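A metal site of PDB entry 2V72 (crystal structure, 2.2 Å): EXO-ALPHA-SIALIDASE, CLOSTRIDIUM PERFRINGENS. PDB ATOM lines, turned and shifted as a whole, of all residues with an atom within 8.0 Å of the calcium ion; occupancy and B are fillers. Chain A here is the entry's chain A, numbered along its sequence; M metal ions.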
ATOM      1  N   GLN A  13       0.224 -10.439 -23.353  1.00  0.00           N
ATOM      2  CA  GLN A  13      -0.406 -11.582 -22.722  1.00  0.00           C
ATOM      3  C   GLN A  13       0.560 -12.760 -22.594  1.00  0.00           C
ATOM      4  O   GLN A  13       0.386 -13.620 -21.723  1.00  0.00           O
ATOM      5  CB  GLN A  13      -1.655 -11.999 -23.498  1.00  0.00           C
ATOM      6  CG  GLN A  13      -2.849 -11.056 -23.362  1.00  0.00           C
ATOM      7  CD  GLN A  13      -4.079 -11.544 -24.106  1.00  0.00           C
ATOM      8  OE1 GLN A  13      -3.993 -11.959 -25.256  1.00  0.00           O
ATOM      9  NE2 GLN A  13      -5.243 -11.469 -23.462  1.00  0.00           N
ATOM     10  N   PRO A  28      -9.609 -23.924 -20.265  1.00  0.00           N
ATOM     11  CA  PRO A  28      -8.711 -23.634 -19.139  1.00  0.00           C
ATOM     12  C   PRO A  28      -8.485 -22.122 -18.941  1.00  0.00           C
ATOM     13  O   PRO A  28      -8.751 -21.337 -19.848  1.00  0.00           O
ATOM     14  CB  PRO A  28      -7.399 -24.295 -19.568  1.00  0.00           C
ATOM     15  CG  PRO A  28      -7.430 -24.250 -21.057  1.00  0.00           C
ATOM     16  CD  PRO A  28      -8.873 -24.390 -21.455  1.00  0.00           C
ATOM     17  N   ALA A  29      -7.990 -21.748 -17.771  1.00  0.00           N
ATOM     18  CA  ALA A  29      -7.635 -20.360 -17.471  1.00  0.00           C
ATOM     19  C   ALA A  29      -6.760 -19.682 -18.530  1.00  0.00           C
ATOM     20  O   ALA A  29      -6.932 -18.488 -18.809  1.00  0.00           O
ATOM     21  CB  ALA A  29      -6.960 -20.291 -16.131  1.00  0.00           C
ATOM     22  N   SER A  30      -5.837 -20.442 -19.128  1.00  0.00           N
ATOM     23  CA  SER A  30      -4.888 -19.950 -20.118  1.00  0.00           C
ATOM     24  C   SER A  30      -5.545 -19.486 -21.411  1.00  0.00           C
ATOM     25  O   SER A  30      -4.984 -18.671 -22.157  1.00  0.00           O
ATOM     26  CB  SER A  30      -3.872 -21.045 -20.438  1.00  0.00           C
ATOM     27  OG  SER A  30      -4.502 -22.185 -21.027  1.00  0.00           O
ATOM     28  N   SER A  31      -6.742 -19.993 -21.666  1.00  0.00           N
ATOM     29  CA  SER A  31      -7.497 -19.617 -22.848  1.00  0.00           C
ATOM     30  C   SER A  31      -8.115 -18.223 -22.722  1.00  0.00           C
ATOM     31  O   SER A  31      -8.621 -17.691 -23.701  1.00  0.00           O
ATOM     32  CB  SER A  31      -8.559 -20.661 -23.147  1.00  0.00           C
ATOM     33  OG  SER A  31      -7.965 -21.789 -23.747  1.00  0.00           O
ATOM     34  N   ALA A  32      -8.055 -17.646 -21.522  1.00  0.00           N
ATOM     35  CA  ALA A  32      -8.495 -16.272 -21.293  1.00  0.00           C
ATOM     36  C   ALA A  32      -7.453 -15.249 -21.755  1.00  0.00           C
ATOM     37  O   ALA A  32      -7.780 -14.077 -21.942  1.00  0.00           O
ATOM     38  CB  ALA A  32      -8.837 -16.064 -19.827  1.00  0.00           C
ATOM     39  N   ILE A  33      -6.215 -15.714 -21.958  1.00  0.00           N
ATOM     40  CA  ILE A  33      -5.095 -14.827 -22.267  1.00  0.00           C
ATOM     41  C   ILE A  33      -4.276 -15.266 -23.495  1.00  0.00           C
ATOM     42  O   ILE A  33      -3.058 -15.089 -23.537  1.00  0.00           O
ATOM     43  CB  ILE A  33      -4.156 -14.624 -21.033  1.00  0.00           C
ATOM     44  CG1 ILE A  33      -3.707 -15.977 -20.442  1.00  0.00           C
ATOM     45  CG2 ILE A  33      -4.858 -13.775 -19.964  1.00  0.00           C
ATOM     46  CD1 ILE A  33      -2.464 -15.907 -19.556  1.00  0.00           C
ATOM     47  N   ASP A  34      -4.954 -15.817 -24.503  1.00  0.00           N
ATOM     48  CA  ASP A  34      -4.261 -16.359 -25.686  1.00  0.00           C
ATOM     49  C   ASP A  34      -4.474 -15.520 -26.957  1.00  0.00           C
ATOM     50  O   ASP A  34      -4.074 -15.928 -28.048  1.00  0.00           O
ATOM     51  CB  ASP A  34      -4.654 -17.823 -25.931  1.00  0.00           C
ATOM     52  CG  ASP A  34      -6.140 -18.015 -26.245  1.00  0.00           C
ATOM     53  OD1 ASP A  34      -6.940 -17.064 -26.070  1.00  0.00           O
ATOM     54  OD2 ASP A  34      -6.515 -19.133 -26.657  1.00  0.00           O
ATOM     55  N   GLY A  35      -5.112 -14.368 -26.805  1.00  0.00           N
ATOM     56  CA  GLY A  35      -5.311 -13.442 -27.914  1.00  0.00           C
ATOM     57  C   GLY A  35      -6.326 -13.888 -28.943  1.00  0.00           C
ATOM     58  O   GLY A  35      -6.399 -13.315 -30.033  1.00  0.00           O
ATOM     59  N   ASN A  36      -7.107 -14.903 -28.588  1.00  0.00           N
ATOM     60  CA  ASN A  36      -8.107 -15.494 -29.472  1.00  0.00           C
ATOM     61  C   ASN A  36      -9.501 -15.408 -28.843  1.00  0.00           C
ATOM     62  O   ASN A  36      -9.734 -15.983 -27.781  1.00  0.00           O
ATOM     63  CB  ASN A  36      -7.750 -16.964 -29.765  1.00  0.00           C
ATOM     64  CG  ASN A  36      -8.594 -17.571 -30.876  1.00  0.00           C
ATOM     65  OD1 ASN A  36      -9.807 -17.404 -30.926  1.00  0.00           O
ATOM     66  ND2 ASN A  36      -7.943 -18.301 -31.776  1.00  0.00           N
ATOM     67  N   ILE A  37     -10.419 -14.703 -29.498  1.00  0.00           N
ATOM     68  CA  ILE A  37     -11.759 -14.505 -28.956  1.00  0.00           C
ATOM     69  C   ILE A  37     -12.684 -15.734 -29.119  1.00  0.00           C
ATOM     70  O   ILE A  37     -13.813 -15.759 -28.592  1.00  0.00           O
ATOM     71  CB  ILE A  37     -12.423 -13.207 -29.517  1.00  0.00           C
ATOM     72  CG1 ILE A  37     -12.600 -13.294 -31.037  1.00  0.00           C
ATOM     73  CG2 ILE A  37     -11.599 -11.975 -29.112  1.00  0.00           C
ATOM     74  CD1 ILE A  37     -12.979 -11.956 -31.726  1.00  0.00           C
ATOM     75  N   ASN A  38     -12.197 -16.757 -29.824  1.00  0.00           N
ATOM     76  CA  ASN A  38     -12.921 -18.021 -29.981  1.00  0.00           C
ATOM     77  C   ASN A  38     -12.660 -19.040 -28.864  1.00  0.00           C
ATOM     78  O   ASN A  38     -13.398 -20.008 -28.733  1.00  0.00           O
ATOM     79  CB  ASN A  38     -12.627 -18.648 -31.348  1.00  0.00           C
ATOM     80  CG  ASN A  38     -13.113 -17.787 -32.510  1.00  0.00           C
ATOM     81  OD1 ASN A  38     -14.140 -17.116 -32.425  1.00  0.00           O
ATOM     82  ND2 ASN A  38     -12.368 -17.804 -33.609  1.00  0.00           N
ATOM     83  N   THR A  39     -11.612 -18.816 -28.074  1.00  0.00           N
ATOM     84  CA  THR A  39     -11.305 -19.660 -26.920  1.00  0.00           C
ATOM     85  C   THR A  39     -11.587 -18.896 -25.631  1.00  0.00           C
ATOM     86  O   THR A  39     -11.228 -17.715 -25.522  1.00  0.00           O
ATOM     87  CB  THR A  39      -9.822 -20.067 -26.884  1.00  0.00           C
ATOM     88  OG1 THR A  39      -9.030 -18.881 -26.787  1.00  0.00           O
ATOM     89  CG2 THR A  39      -9.416 -20.840 -28.139  1.00  0.00           C
ATOM     90  N   MET A  40     -12.194 -19.569 -24.668  1.00  0.00           N
ATOM     91  CA  MET A  40     -12.533 -18.943 -23.378  1.00  0.00           C
ATOM     92  C   MET A  40     -12.073 -19.740 -22.160  1.00  0.00           C
ATOM     93  O   MET A  40     -11.852 -20.953 -22.252  1.00  0.00           O
ATOM     94  CB  MET A  40     -14.045 -18.744 -23.284  1.00  0.00           C
ATOM     95  CG  MET A  40     -14.844 -20.027 -23.215  1.00  0.00           C
ATOM     96  SD  MET A  40     -16.601 -19.690 -23.321  1.00  0.00           S
ATOM     97  CE  MET A  40     -16.813 -19.731 -25.096  1.00  0.00           C
ATOM     98  N   TRP A  41     -11.936 -19.038 -21.028  1.00  0.00           N
ATOM     99  CA  TRP A  41     -11.950 -19.676 -19.730  1.00  0.00           C
ATOM    100  C   TRP A  41     -13.418 -19.831 -19.344  1.00  0.00           C
ATOM    101  O   TRP A  41     -14.216 -18.931 -19.560  1.00  0.00           O
ATOM    102  CB  TRP A  41     -11.211 -18.833 -18.660  1.00  0.00           C
ATOM    103  CG  TRP A  41     -11.558 -19.274 -17.258  1.00  0.00           C
ATOM    104  CD1 TRP A  41     -11.248 -20.480 -16.687  1.00  0.00           C
ATOM    105  CD2 TRP A  41     -12.322 -18.548 -16.275  1.00  0.00           C
ATOM    106  NE1 TRP A  41     -11.759 -20.535 -15.407  1.00  0.00           N
ATOM    107  CE2 TRP A  41     -12.411 -19.372 -15.122  1.00  0.00           C
ATOM    108  CE3 TRP A  41     -12.918 -17.272 -16.248  1.00  0.00           C
ATOM    109  CZ2 TRP A  41     -13.073 -18.969 -13.964  1.00  0.00           C
ATOM    110  CZ3 TRP A  41     -13.569 -16.878 -15.092  1.00  0.00           C
ATOM    111  CH2 TRP A  41     -13.647 -17.720 -13.960  1.00  0.00           C
ATOM    112  N   THR A  71     -13.379  -9.388 -22.089  1.00  0.00           N
ATOM    113  CA  THR A  71     -14.119  -9.813 -23.281  1.00  0.00           C
ATOM    114  C   THR A  71     -14.933 -11.083 -23.000  1.00  0.00           C
ATOM    115  O   THR A  71     -14.366 -12.150 -22.744  1.00  0.00           O
ATOM    116  CB  THR A  71     -13.150 -10.084 -24.451  1.00  0.00           C
ATOM    117  OG1 THR A  71     -12.267  -8.968 -24.613  1.00  0.00           O
ATOM    118  CG2 THR A  71     -13.908 -10.350 -25.754  1.00  0.00           C
ATOM    119  N   ILE A 136     -14.784 -16.063 -19.594  1.00  0.00           N
ATOM    120  CA  ILE A 136     -14.052 -14.917 -20.130  1.00  0.00           C
ATOM    121  C   ILE A 136     -13.270 -15.450 -21.320  1.00  0.00           C
ATOM    122  O   ILE A 136     -12.452 -16.360 -21.189  1.00  0.00           O
ATOM    123  CB  ILE A 136     -13.064 -14.292 -19.089  1.00  0.00           C
ATOM    124  CG1 ILE A 136     -13.820 -13.586 -17.955  1.00  0.00           C
ATOM    125  CG2 ILE A 136     -12.112 -13.308 -19.763  1.00  0.00           C
ATOM    126  CD1 ILE A 136     -12.935 -13.160 -16.771  1.00  0.00           C
ATOM    127  N   ALA A 137     -13.521 -14.883 -22.496  1.00  0.00           N
ATOM    128  CA  ALA A 137     -12.825 -15.304 -23.715  1.00  0.00           C
ATOM    129  C   ALA A 137     -11.465 -14.628 -23.855  1.00  0.00           C
ATOM    130  O   ALA A 137     -10.506 -15.246 -24.311  1.00  0.00           O
ATOM    131  CB  ALA A 137     -13.700 -15.069 -24.963  1.00  0.00           C
ATOM    132  N   GLU A 138     -11.388 -13.360 -23.435  1.00  0.00           N
ATOM    133  CA  GLU A 138     -10.126 -12.606 -23.446  1.00  0.00           C
ATOM    134  C   GLU A 138     -10.019 -11.617 -22.286  1.00  0.00           C
ATOM    135  O   GLU A 138     -11.009 -10.982 -21.901  1.00  0.00           O
ATOM    136  CB  GLU A 138      -9.915 -11.869 -24.764  1.00  0.00           C
ATOM    137  CG  GLU A 138      -9.345 -12.692 -25.900  1.00  0.00           C
ATOM    138  CD  GLU A 138      -7.998 -13.292 -25.562  1.00  0.00           C
ATOM    139  OE1 GLU A 138      -7.030 -12.523 -25.343  1.00  0.00           O
ATOM    140  OE2 GLU A 138      -7.910 -14.525 -25.524  1.00  0.00           O
ATOM    141  N   LEU A 139      -8.822 -11.494 -21.734  1.00  0.00           N
ATOM    142  CA  LEU A 139      -8.536 -10.542 -20.684  1.00  0.00           C
ATOM    143  C   LEU A 139      -7.255  -9.793 -21.017  1.00  0.00           C
ATOM    144  O   LEU A 139      -6.207 -10.399 -21.245  1.00  0.00           O
ATOM    145  CB  LEU A 139      -8.406 -11.236 -19.319  1.00  0.00           C
ATOM    146  CG  LEU A 139      -8.347 -10.239 -18.162  1.00  0.00           C
ATOM    147  CD1 LEU A 139      -9.221 -10.669 -17.005  1.00  0.00           C
ATOM    148  CD2 LEU A 139      -6.908  -9.965 -17.713  1.00  0.00           C
HETATM  149 CA    CA M   1      -9.161 -16.587 -25.646  1.00  0.00          CA
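The backbone NH (N) of Ala 137 sits at hydrogen-bond distance from the backbone carbonyl oxygen (O) of Thr 71 (2.9 Å).
The side-chain carboxylate (OE1) of Glu 138 sits at hydrogen-bond distance from the side-chain amide nitrogen (NE2) of Gln 13 (2.8 Å).
The backbone NH (N) of Gly 35 is in hydrogen-bond range of the side-chain carboxylate (OE1) of Glu 138, at 3.0 Å.
O of Glu 138 sits at hydrogen-bond distance from N of Thr 71 (2.9 Å).
The side-chain amide oxygen of Asn 36 lies within hydrogen-bond range of the backbone NH of Asn 38, at 2.7 Å.
Six residues have an atom within 4 Å of the calcium ion: Ser 31, Asp 34, Asn 36, Thr 39, Ala 137 and Glu 138.
Along chain A the residues within 4 Å of the calcium ion span positions 31 to 138.
The calcium ion is bound by O of Asn 36.
The calcium ion is bound by O of Ser 31, at 2.3 Å.
OD1 of Asp 34 binds the calcium ion (2.3 Å).
The backbone carbonyl oxygen (O) of Ala 137 is bound to the calcium ion (2.3 Å).
O of Thr 39 binds the calcium ion (2.4 Å).
The side-chain carboxylate (OE2) of Glu 138 binds the calcium ion.
OG1 of Thr 39 binds the calcium ion, at 2.6 Å.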
